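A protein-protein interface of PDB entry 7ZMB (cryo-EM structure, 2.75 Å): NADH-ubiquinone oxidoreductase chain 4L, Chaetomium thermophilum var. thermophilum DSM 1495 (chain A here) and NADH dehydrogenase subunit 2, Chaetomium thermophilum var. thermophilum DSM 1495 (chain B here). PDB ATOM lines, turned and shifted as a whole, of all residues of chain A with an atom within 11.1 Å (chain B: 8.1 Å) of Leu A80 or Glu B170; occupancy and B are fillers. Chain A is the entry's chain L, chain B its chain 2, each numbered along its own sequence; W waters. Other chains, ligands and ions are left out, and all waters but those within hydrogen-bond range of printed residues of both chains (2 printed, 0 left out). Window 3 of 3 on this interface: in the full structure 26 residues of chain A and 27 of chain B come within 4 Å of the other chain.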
ATOM      1  N   ILE A  22      30.234  -9.569  12.420  1.00  0.00           N
ATOM      2  CA  ILE A  22      31.500 -10.223  12.112  1.00  0.00           C
ATOM      3  C   ILE A  22      32.653  -9.236  11.951  1.00  0.00           C
ATOM      4  O   ILE A  22      33.816  -9.634  12.086  1.00  0.00           O
ATOM      5  CB  ILE A  22      31.327 -11.101  10.860  1.00  0.00           C
ATOM      6  CG1 ILE A  22      30.159 -12.066  11.054  1.00  0.00           C
ATOM      7  CG2 ILE A  22      32.589 -11.886  10.536  1.00  0.00           C
ATOM      8  CD1 ILE A  22      29.446 -12.429   9.780  1.00  0.00           C
ATOM      9  N   GLY A  72      37.706  -9.082   2.592  1.00  0.00           N
ATOM     10  CA  GLY A  72      37.337  -9.596   1.284  1.00  0.00           C
ATOM     11  C   GLY A  72      36.363 -10.757   1.359  1.00  0.00           C
ATOM     12  O   GLY A  72      35.416 -10.833   0.574  1.00  0.00           O
ATOM     13  N   ILE A  73      36.585 -11.680   2.293  1.00  0.00           N
ATOM     14  CA  ILE A  73      35.676 -12.808   2.451  1.00  0.00           C
ATOM     15  C   ILE A  73      34.346 -12.340   3.015  1.00  0.00           C
ATOM     16  O   ILE A  73      33.279 -12.837   2.634  1.00  0.00           O
ATOM     17  CB  ILE A  73      36.323 -13.897   3.325  1.00  0.00           C
ATOM     18  CG1 ILE A  73      37.360 -14.668   2.510  1.00  0.00           C
ATOM     19  CG2 ILE A  73      35.274 -14.854   3.857  1.00  0.00           C
ATOM     20  CD1 ILE A  73      38.279 -15.528   3.322  1.00  0.00           C
ATOM     21  N   LEU A  74      34.389 -11.372   3.931  1.00  0.00           N
ATOM     22  CA  LEU A  74      33.174 -10.825   4.518  1.00  0.00           C
ATOM     23  C   LEU A  74      32.286 -10.189   3.456  1.00  0.00           C
ATOM     24  O   LEU A  74      31.065 -10.378   3.460  1.00  0.00           O
ATOM     25  CB  LEU A  74      33.556  -9.813   5.590  1.00  0.00           C
ATOM     26  CG  LEU A  74      32.559  -9.374   6.650  1.00  0.00           C
ATOM     27  CD1 LEU A  74      31.725 -10.549   7.147  1.00  0.00           C
ATOM     28  CD2 LEU A  74      33.338  -8.739   7.775  1.00  0.00           C
ATOM     29  N   VAL A  75      32.867  -9.435   2.531  1.00  0.00           N
ATOM     30  CA  VAL A  75      32.082  -8.827   1.414  1.00  0.00           C
ATOM     31  C   VAL A  75      31.410  -9.936   0.594  1.00  0.00           C
ATOM     32  O   VAL A  75      30.204  -9.807   0.319  1.00  0.00           O
ATOM     33  CB  VAL A  75      32.935  -7.880   0.545  1.00  0.00           C
ATOM     34  CG1 VAL A  75      32.305  -7.592  -0.805  1.00  0.00           C
ATOM     35  CG2 VAL A  75      33.239  -6.587   1.272  1.00  0.00           C
ATOM     36  N   ALA A  76      32.176 -10.953   0.179  1.00  0.00           N
ATOM     37  CA  ALA A  76      31.636 -12.100  -0.588  1.00  0.00           C
ATOM     38  C   ALA A  76      30.422 -12.688   0.129  1.00  0.00           C
ATOM     39  O   ALA A  76      29.380 -12.865  -0.517  1.00  0.00           O
ATOM     40  CB  ALA A  76      32.722 -13.117  -0.802  1.00  0.00           C
ATOM     41  N   PHE A  77      30.571 -12.987   1.416  1.00  0.00           N
ATOM     42  CA  PHE A  77      29.472 -13.554   2.233  1.00  0.00           C
ATOM     43  C   PHE A  77      28.279 -12.595   2.279  1.00  0.00           C
ATOM     44  O   PHE A  77      27.169 -13.079   2.069  1.00  0.00           O
ATOM     45  CB  PHE A  77      30.031 -13.854   3.631  1.00  0.00           C
ATOM     46  CG  PHE A  77      29.052 -14.163   4.733  1.00  0.00           C
ATOM     47  CD1 PHE A  77      28.636 -15.462   4.973  1.00  0.00           C
ATOM     48  CD2 PHE A  77      28.600 -13.162   5.576  1.00  0.00           C
ATOM     49  CE1 PHE A  77      27.757 -15.744   6.005  1.00  0.00           C
ATOM     50  CE2 PHE A  77      27.717 -13.445   6.606  1.00  0.00           C
ATOM     51  CZ  PHE A  77      27.302 -14.737   6.822  1.00  0.00           C
ATOM     52  N   TYR A  78      28.503 -11.294   2.502  1.00  0.00           N
ATOM     53  CA  TYR A  78      27.410 -10.286   2.603  1.00  0.00           C
ATOM     54  C   TYR A  78      26.651 -10.171   1.280  1.00  0.00           C
ATOM     55  O   TYR A  78      25.439 -10.020   1.301  1.00  0.00           O
ATOM     56  CB  TYR A  78      27.957  -8.922   3.030  1.00  0.00           C
ATOM     57  CG  TYR A  78      26.954  -7.799   3.090  1.00  0.00           C
ATOM     58  CD1 TYR A  78      26.696  -7.009   1.981  1.00  0.00           C
ATOM     59  CD2 TYR A  78      26.278  -7.508   4.261  1.00  0.00           C
ATOM     60  CE1 TYR A  78      25.784  -5.973   2.029  1.00  0.00           C
ATOM     61  CE2 TYR A  78      25.368  -6.469   4.330  1.00  0.00           C
ATOM     62  CZ  TYR A  78      25.121  -5.699   3.210  1.00  0.00           C
ATOM     63  OH  TYR A  78      24.221  -4.678   3.268  1.00  0.00           O
ATOM     64  N   ARG A  79      27.354 -10.234   0.159  1.00  0.00           N
ATOM     65  CA  ARG A  79      26.668 -10.045  -1.138  1.00  0.00           C
ATOM     66  C   ARG A  79      25.593 -11.116  -1.225  1.00  0.00           C
ATOM     67  O   ARG A  79      24.520 -10.825  -1.753  1.00  0.00           O
ATOM     68  CB  ARG A  79      27.642 -10.158  -2.308  1.00  0.00           C
ATOM     69  CG  ARG A  79      28.649  -9.025  -2.418  1.00  0.00           C
ATOM     70  CD  ARG A  79      29.026  -8.842  -3.872  1.00  0.00           C
ATOM     71  NE  ARG A  79      30.410  -8.450  -4.083  1.00  0.00           N
ATOM     72  CZ  ARG A  79      30.845  -7.199  -4.122  1.00  0.00           C
ATOM     73  NH1 ARG A  79      32.125  -6.959  -4.334  1.00  0.00           N
ATOM     74  NH2 ARG A  79      30.005  -6.196  -3.948  1.00  0.00           N
ATOM     75  N   LEU A  80      25.885 -12.317  -0.740  1.00  0.00           N
ATOM     76  CA  LEU A  80      24.912 -13.418  -0.874  1.00  0.00           C
ATOM     77  C   LEU A  80      23.929 -13.473   0.308  1.00  0.00           C
ATOM     78  O   LEU A  80      22.720 -13.511   0.044  1.00  0.00           O
ATOM     79  CB  LEU A  80      25.734 -14.686  -1.055  1.00  0.00           C
ATOM     80  CG  LEU A  80      26.580 -14.712  -2.326  1.00  0.00           C
ATOM     81  CD1 LEU A  80      27.670 -15.765  -2.242  1.00  0.00           C
ATOM     82  CD2 LEU A  80      25.718 -14.932  -3.556  1.00  0.00           C
ATOM     83  N   ARG A  81      24.410 -13.394   1.548  1.00  0.00           N
ATOM     84  CA  ARG A  81      23.532 -13.473   2.744  1.00  0.00           C
ATOM     85  C   ARG A  81      22.758 -12.159   2.928  1.00  0.00           C
ATOM     86  O   ARG A  81      21.563 -12.228   3.278  1.00  0.00           O
ATOM     87  CB  ARG A  81      24.348 -13.824   3.993  1.00  0.00           C
ATOM     88  CG  ARG A  81      23.494 -14.054   5.231  1.00  0.00           C
ATOM     89  CD  ARG A  81      23.961 -15.237   6.051  1.00  0.00           C
ATOM     90  NE  ARG A  81      24.436 -16.329   5.212  1.00  0.00           N
ATOM     91  CZ  ARG A  81      23.687 -17.339   4.787  1.00  0.00           C
ATOM     92  NH1 ARG A  81      22.410 -17.404   5.123  1.00  0.00           N
ATOM     93  NH2 ARG A  81      24.218 -18.279   4.027  1.00  0.00           N
ATOM     94  N   GLY A  82      23.413 -11.010   2.739  1.00  0.00           N
ATOM     95  CA  GLY A  82      22.760  -9.696   2.908  1.00  0.00           C
ATOM     96  C   GLY A  82      22.839  -9.112   4.308  1.00  0.00           C
ATOM     97  O   GLY A  82      22.452  -7.947   4.476  1.00  0.00           O
ATOM     98  N   SER A  83      23.282  -9.885   5.291  1.00  0.00           N
ATOM     99  CA  SER A  83      23.493  -9.367   6.664  1.00  0.00           C
ATOM    100  C   SER A  83      24.797  -9.969   7.170  1.00  0.00           C
ATOM    101  O   SER A  83      25.002 -11.167   6.919  1.00  0.00           O
ATOM    102  CB  SER A  83      22.354  -9.760   7.560  1.00  0.00           C
ATOM    103  OG  SER A  83      22.554  -9.298   8.882  1.00  0.00           O
ATOM    104  N   ILE A  84      25.661  -9.185   7.814  1.00  0.00           N
ATOM    105  CA  ILE A  84      26.869  -9.805   8.439  1.00  0.00           C
ATOM    106  C   ILE A  84      26.619  -9.769   9.937  1.00  0.00           C
ATOM    107  O   ILE A  84      27.584  -9.844  10.703  1.00  0.00           O
ATOM    108  CB  ILE A  84      28.181  -9.129   8.011  1.00  0.00           C
ATOM    109  CG1 ILE A  84      28.255  -7.675   8.487  1.00  0.00           C
ATOM    110  CG2 ILE A  84      28.388  -9.244   6.514  1.00  0.00           C
ATOM    111  CD1 ILE A  84      29.645  -7.105   8.476  1.00  0.00           C
ATOM    112  N   ALA A  85      25.358  -9.628  10.322  1.00  0.00           N
ATOM    113  CA  ALA A  85      24.957  -9.654  11.717  1.00  0.00           C
ATOM    114  C   ALA A  85      24.887 -11.101  12.167  1.00  0.00           C
ATOM    115  O   ALA A  85      24.371 -11.960  11.441  1.00  0.00           O
ATOM    116  CB  ALA A  85      23.609  -8.964  11.913  1.00  0.00           C
ATOM    117  N   GLU A  87      23.385 -13.949  14.484  1.00  0.00           N
ATOM    118  CA  GLU A  87      22.022 -14.056  14.984  1.00  0.00           C
ATOM    119  C   GLU A  87      21.946 -15.034  16.144  1.00  0.00           C
ATOM    120  O   GLU A  87      22.393 -16.181  16.029  1.00  0.00           O
ATOM    121  CB  GLU A  87      21.067 -14.490  13.868  1.00  0.00           C
ATOM    122  CG  GLU A  87      20.917 -13.469  12.753  1.00  0.00           C
ATOM    123  CD  GLU A  87      19.776 -13.797  11.811  1.00  0.00           C
ATOM    124  OE1 GLU A  87      18.895 -14.595  12.193  1.00  0.00           O
ATOM    125  OE2 GLU A  87      19.760 -13.258  10.684  1.00  0.00           O
ATOM    126  N   THR B 164      36.710 -20.038  -0.327  1.00  0.00           N
ATOM    127  CA  THR B 164      35.803 -18.916  -0.692  1.00  0.00           C
ATOM    128  C   THR B 164      35.896 -18.608  -2.189  1.00  0.00           C
ATOM    129  O   THR B 164      35.195 -17.693  -2.623  1.00  0.00           O
ATOM    130  CB  THR B 164      36.197 -17.648   0.080  1.00  0.00           C
ATOM    131  OG1 THR B 164      36.260 -17.967   1.469  1.00  0.00           O
ATOM    132  CG2 THR B 164      35.246 -16.493  -0.147  1.00  0.00           C
ATOM    133  N   TYR B 166      34.763 -20.003  -4.764  1.00  0.00           N
ATOM    134  CA  TYR B 166      33.438 -20.099  -5.448  1.00  0.00           C
ATOM    135  C   TYR B 166      32.654 -18.958  -4.805  1.00  0.00           C
ATOM    136  O   TYR B 166      32.042 -19.194  -3.755  1.00  0.00           O
ATOM    137  CB  TYR B 166      32.825 -21.487  -5.270  1.00  0.00           C
ATOM    138  CG  TYR B 166      33.397 -22.560  -6.159  1.00  0.00           C
ATOM    139  CD1 TYR B 166      34.708 -22.982  -6.026  1.00  0.00           C
ATOM    140  CD2 TYR B 166      32.617 -23.172  -7.125  1.00  0.00           C
ATOM    141  CE1 TYR B 166      35.234 -23.975  -6.833  1.00  0.00           C
ATOM    142  CE2 TYR B 166      33.125 -24.169  -7.938  1.00  0.00           C
ATOM    143  CZ  TYR B 166      34.439 -24.570  -7.794  1.00  0.00           C
ATOM    144  OH  TYR B 166      34.941 -25.551  -8.595  1.00  0.00           O
ATOM    145  N   ARG B 167      32.639 -17.782  -5.424  1.00  0.00           N
ATOM    146  CA  ARG B 167      32.111 -16.555  -4.777  1.00  0.00           C
ATOM    147  C   ARG B 167      30.617 -16.397  -5.015  1.00  0.00           C
ATOM    148  O   ARG B 167      30.016 -15.511  -4.409  1.00  0.00           O
ATOM    149  CB  ARG B 167      32.859 -15.391  -5.427  1.00  0.00           C
ATOM    150  CG  ARG B 167      32.913 -15.515  -6.941  1.00  0.00           C
ATOM    151  CD  ARG B 167      33.595 -14.314  -7.539  1.00  0.00           C
ATOM    152  NE  ARG B 167      32.900 -13.108  -7.133  1.00  0.00           N
ATOM    153  CZ  ARG B 167      33.424 -11.903  -7.251  1.00  0.00           C
ATOM    154  NH1 ARG B 167      32.743 -10.837  -6.868  1.00  0.00           N
ATOM    155  NH2 ARG B 167      34.640 -11.780  -7.744  1.00  0.00           N
ATOM    156  N   ASN B 168      30.067 -17.228  -5.891  1.00  0.00           N
ATOM    157  CA  ASN B 168      28.624 -17.117  -6.222  1.00  0.00           C
ATOM    158  C   ASN B 168      27.880 -18.222  -5.482  1.00  0.00           C
ATOM    159  O   ASN B 168      26.670 -18.350  -5.706  1.00  0.00           O
ATOM    160  CB  ASN B 168      28.456 -17.070  -7.737  1.00  0.00           C
ATOM    161  CG  ASN B 168      29.312 -16.012  -8.390  1.00  0.00           C
ATOM    162  OD1 ASN B 168      29.504 -14.932  -7.837  1.00  0.00           O
ATOM    163  ND2 ASN B 168      29.822 -16.308  -9.573  1.00  0.00           N
ATOM    164  N   SER B 169      28.598 -18.942  -4.625  1.00  0.00           N
ATOM    165  CA  SER B 169      27.980 -19.981  -3.773  1.00  0.00           C
ATOM    166  C   SER B 169      27.806 -19.416  -2.366  1.00  0.00           C
ATOM    167  O   SER B 169      28.820 -19.054  -1.762  1.00  0.00           O
ATOM    168  CB  SER B 169      28.835 -21.206  -3.759  1.00  0.00           C
ATOM    169  OG  SER B 169      28.361 -22.148  -2.817  1.00  0.00           O
ATOM    170  N   GLU B 170      26.570 -19.336  -1.871  1.00  0.00           N
ATOM    171  CA  GLU B 170      26.308 -18.889  -0.472  1.00  0.00           C
ATOM    172  C   GLU B 170      26.840 -19.946   0.489  1.00  0.00           C
ATOM    173  O   GLU B 170      27.111 -19.608   1.643  1.00  0.00           O
ATOM    174  CB  GLU B 170      24.828 -18.604  -0.217  1.00  0.00           C
ATOM    175  CG  GLU B 170      23.906 -19.760  -0.556  1.00  0.00           C
ATOM    176  CD  GLU B 170      23.521 -19.859  -2.024  1.00  0.00           C
ATOM    177  OE1 GLU B 170      24.137 -20.672  -2.744  1.00  0.00           O
ATOM    178  OE2 GLU B 170      22.614 -19.116  -2.443  1.00  0.00           O
ATOM    179  N   LEU B 171      27.056 -21.161  -0.008  1.00  0.00           N
ATOM    180  CA  LEU B 171      27.503 -22.268   0.865  1.00  0.00           C
ATOM    181  C   LEU B 171      29.021 -22.201   1.014  1.00  0.00           C
ATOM    182  O   LEU B 171      29.508 -22.543   2.089  1.00  0.00           O
ATOM    183  CB  LEU B 171      27.032 -23.615   0.311  1.00  0.00           C
ATOM    184  CG  LEU B 171      25.662 -24.084   0.772  1.00  0.00           C
ATOM    185  CD1 LEU B 171      25.432 -25.525   0.352  1.00  0.00           C
ATOM    186  CD2 LEU B 171      25.549 -23.947   2.275  1.00  0.00           C
ATOM    187  N   SER B 172      29.729 -21.736  -0.018  1.00  0.00           N
ATOM    188  CA  SER B 172      31.180 -21.641   0.082  1.00  0.00           C
ATOM    189  C   SER B 172      31.610 -20.403   0.849  1.00  0.00           C
ATOM    190  O   SER B 172      32.575 -20.453   1.616  1.00  0.00           O
ATOM    191  CB  SER B 172      31.815 -21.638  -1.304  1.00  0.00           C
ATOM    192  OG  SER B 172      31.697 -22.908  -1.892  1.00  0.00           O
ATOM    193  N   THR B 173      30.870 -19.330   0.662  1.00  0.00           N
ATOM    194  CA  THR B 173      31.158 -18.054   1.352  1.00  0.00           C
ATOM    195  C   THR B 173      30.995 -18.298   2.844  1.00  0.00           C
ATOM    196  O   THR B 173      31.763 -17.728   3.608  1.00  0.00           O
ATOM    197  CB  THR B 173      30.384 -16.896   0.720  1.00  0.00           C
ATOM    198  OG1 THR B 173      29.000 -17.235   0.661  1.00  0.00           O
ATOM    199  CG2 THR B 173      30.904 -16.548  -0.656  1.00  0.00           C
ATOM    200  N   THR B 174      29.987 -19.085   3.204  1.00  0.00           N
ATOM    201  CA  THR B 174      29.725 -19.412   4.623  1.00  0.00           C
ATOM    202  C   THR B 174      30.823 -20.312   5.179  1.00  0.00           C
ATOM    203  O   THR B 174      31.353 -19.975   6.241  1.00  0.00           O
ATOM    204  CB  THR B 174      28.300 -19.955   4.796  1.00  0.00           C
ATOM    205  OG1 THR B 174      27.396 -18.939   4.366  1.00  0.00           O
ATOM    206  CG2 THR B 174      27.987 -20.316   6.231  1.00  0.00           C
ATOM    207  N   GLY B 175      31.210 -21.336   4.423  1.00  0.00           N
ATOM    208  CA  GLY B 175      32.263 -22.278   4.841  1.00  0.00           C
ATOM    209  C   GLY B 175      33.571 -21.541   4.888  1.00  0.00           C
ATOM    210  O   GLY B 175      34.306 -21.704   5.865  1.00  0.00           O
ATOM    211  N   GLY B 176      33.818 -20.711   3.882  1.00  0.00           N
ATOM    212  CA  GLY B 176      34.999 -19.871   3.920  1.00  0.00           C
ATOM    213  C   GLY B 176      35.021 -18.946   5.122  1.00  0.00           C
ATOM    214  O   GLY B 176      36.057 -18.769   5.762  1.00  0.00           O
ATOM    215  N   LEU B 177      33.874 -18.356   5.454  1.00  0.00           N
ATOM    216  CA  LEU B 177      33.834 -17.394   6.547  1.00  0.00           C
ATOM    217  C   LEU B 177      34.067 -18.065   7.894  1.00  0.00           C
ATOM    218  O   LEU B 177      34.799 -17.533   8.732  1.00  0.00           O
ATOM    219  CB  LEU B 177      32.504 -16.646   6.539  1.00  0.00           C
ATOM    220  CG  LEU B 177      32.407 -15.510   7.550  1.00  0.00           C
ATOM    221  CD1 LEU B 177      33.256 -14.340   7.097  1.00  0.00           C
ATOM    222  CD2 LEU B 177      30.980 -15.095   7.738  1.00  0.00           C
ATOM    223  N   ALA B 270      30.246 -27.721   3.340  1.00  0.00           N
ATOM    224  CA  ALA B 270      29.756 -26.504   2.704  1.00  0.00           C
ATOM    225  C   ALA B 270      30.498 -26.151   1.420  1.00  0.00           C
ATOM    226  O   ALA B 270      29.887 -25.619   0.489  1.00  0.00           O
ATOM    227  CB  ALA B 270      29.839 -25.333   3.686  1.00  0.00           C
ATOM    228  N   LEU B 405      20.894 -28.327  -2.078  1.00  0.00           N
ATOM    229  CA  LEU B 405      21.385 -26.991  -2.395  1.00  0.00           C
ATOM    230  C   LEU B 405      22.801 -27.075  -2.937  1.00  0.00           C
ATOM    231  O   LEU B 405      23.603 -27.880  -2.460  1.00  0.00           O
ATOM    232  CB  LEU B 405      21.377 -26.092  -1.163  1.00  0.00           C
ATOM    233  CG  LEU B 405      20.139 -26.126  -0.279  1.00  0.00           C
ATOM    234  CD1 LEU B 405      20.296 -25.129   0.854  1.00  0.00           C
ATOM    235  CD2 LEU B 405      18.894 -25.830  -1.096  1.00  0.00           C
ATOM    236  N   ASP B 406      23.113 -26.220  -3.911  1.00  0.00           N
ATOM    237  CA  ASP B 406      24.394 -26.237  -4.617  1.00  0.00           C
ATOM    238  C   ASP B 406      24.728 -27.639  -5.117  1.00  0.00           C
ATOM    239  O   ASP B 406      25.758 -28.225  -4.785  1.00  0.00           O
ATOM    240  CB  ASP B 406      25.529 -25.674  -3.749  1.00  0.00           C
ATOM    241  CG  ASP B 406      25.624 -24.156  -3.809  1.00  0.00           C
ATOM    242  OD1 ASP B 406      25.285 -23.574  -4.862  1.00  0.00           O
ATOM    243  OD2 ASP B 406      26.049 -23.537  -2.811  1.00  0.00           O
ATOM    244  N   ASN B 409      28.091 -27.896  -7.171  1.00  0.00           N
ATOM    245  CA  ASN B 409      29.355 -27.896  -6.450  1.00  0.00           C
ATOM    246  C   ASN B 409      29.561 -29.151  -5.622  1.00  0.00           C
ATOM    247  O   ASN B 409      30.703 -29.565  -5.412  1.00  0.00           O
ATOM    248  CB  ASN B 409      29.442 -26.666  -5.544  1.00  0.00           C
ATOM    249  CG  ASN B 409      29.614 -25.388  -6.318  1.00  0.00           C
ATOM    250  OD1 ASN B 409      30.099 -25.394  -7.444  1.00  0.00           O
ATOM    251  ND2 ASN B 409      29.218 -24.277  -5.718  1.00  0.00           N
HETATM  252  O   HOH W   1      26.739 -16.123   2.353  1.00  0.00           O
HETATM  253  O   HOH W   2      29.253 -12.686  -3.797  1.00  0.00           O
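The backbone carbonyl oxygen (O) of Ile A84 sits at hydrogen-bond distance from the backbone NH (N) of Ile A22.
The side-chain hydroxyl (OG1) of Thr B173 lies within hydrogen-bond range of the backbone carbonyl oxygen (O) of Glu B170, at 3.2 Å.
The side-chain hydroxyl (OG) of Ser B169 lies close to the backbone NH (N) of Leu B171 (3.3 Å).
The backbone carbonyl oxygen (O) of Ser B169 sits at hydrogen-bond distance from the side-chain hydroxyl (OG1) of Thr B173 (3.0 Å).
The backbone carbonyl oxygen (O) of Glu B170 lies within hydrogen-bond range of the side-chain hydroxyl (OG1) of Thr B174, at 2.8 Å.
OG of Ser B169 sits at hydrogen-bond distance from OD2 of Asp B406.
Of the 17 printed residues of chain B, 7 touch a printed residue of chain A.
Hydrophobic or aromatic side chains of chain B within 4 Å of the printed part of chain A: Leu B177.
Among the printed residues, no Asp or Glu carboxylate lies within 4 Å of a Lys or Arg side-chain nitrogen of the other chain.
Among the printed residues, pairs that only touch across the chains: Ile A22 with Leu B177, Ile A73 with Thr B164, Ile A73 with Leu B177, Ala A76 with Thr B173, Phe A77 with Thr B173, Phe A77 with Thr B174, Phe A77 with Leu B177, Leu A80 with Arg B167, Leu A80 with Ser B169, Leu A80 with Glu B170, Leu A80 with Thr B173 and Arg A81 with Glu B170.
The guanidinium group (NH2) of Arg A81 is in hydrogen-bond range of the side-chain hydroxyl (OG1) of Thr B174 (3.3 Å).
Water W2 lies within hydrogen-bond range of the backbone carbonyl oxygen (O) of Arg B167 and the backbone carbonyl oxygen (O) of Ala A76.
Water W1 lies within hydrogen-bond range of OG1 of Thr B173 (3.0 Å) and O of Phe A77 (3.1 Å).
Val A75 touches none of the printed residues of chain B.
Of the printed residues of chain B, Leu A80 touches Arg B167, Ser B169, Glu B170 and Thr B173.
Of the printed residues of chain A, Arg B167 touches Leu A80.
Ser B169 touches one residue of chain A.
Of chain A, only Leu A80 (3.8 Å) and Arg A81 (3.98 Å) come within 4 Å of Glu B170.
No residue of chain A comes within 4 Å of Ser B172.
Thr B174 touches just these residues of chain A: Phe A77 (3.6 Å) and Arg A81 (3.3 Å).
Of the printed residues of chain A, Leu B177 touches Ile A22 (3.7 Å), Ile A73 (3.9 Å) and Phe A77 (3.6 Å).
The nearest printed residue of chain B that does not touch Ala A76 is Thr B164 (4.3 Å).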
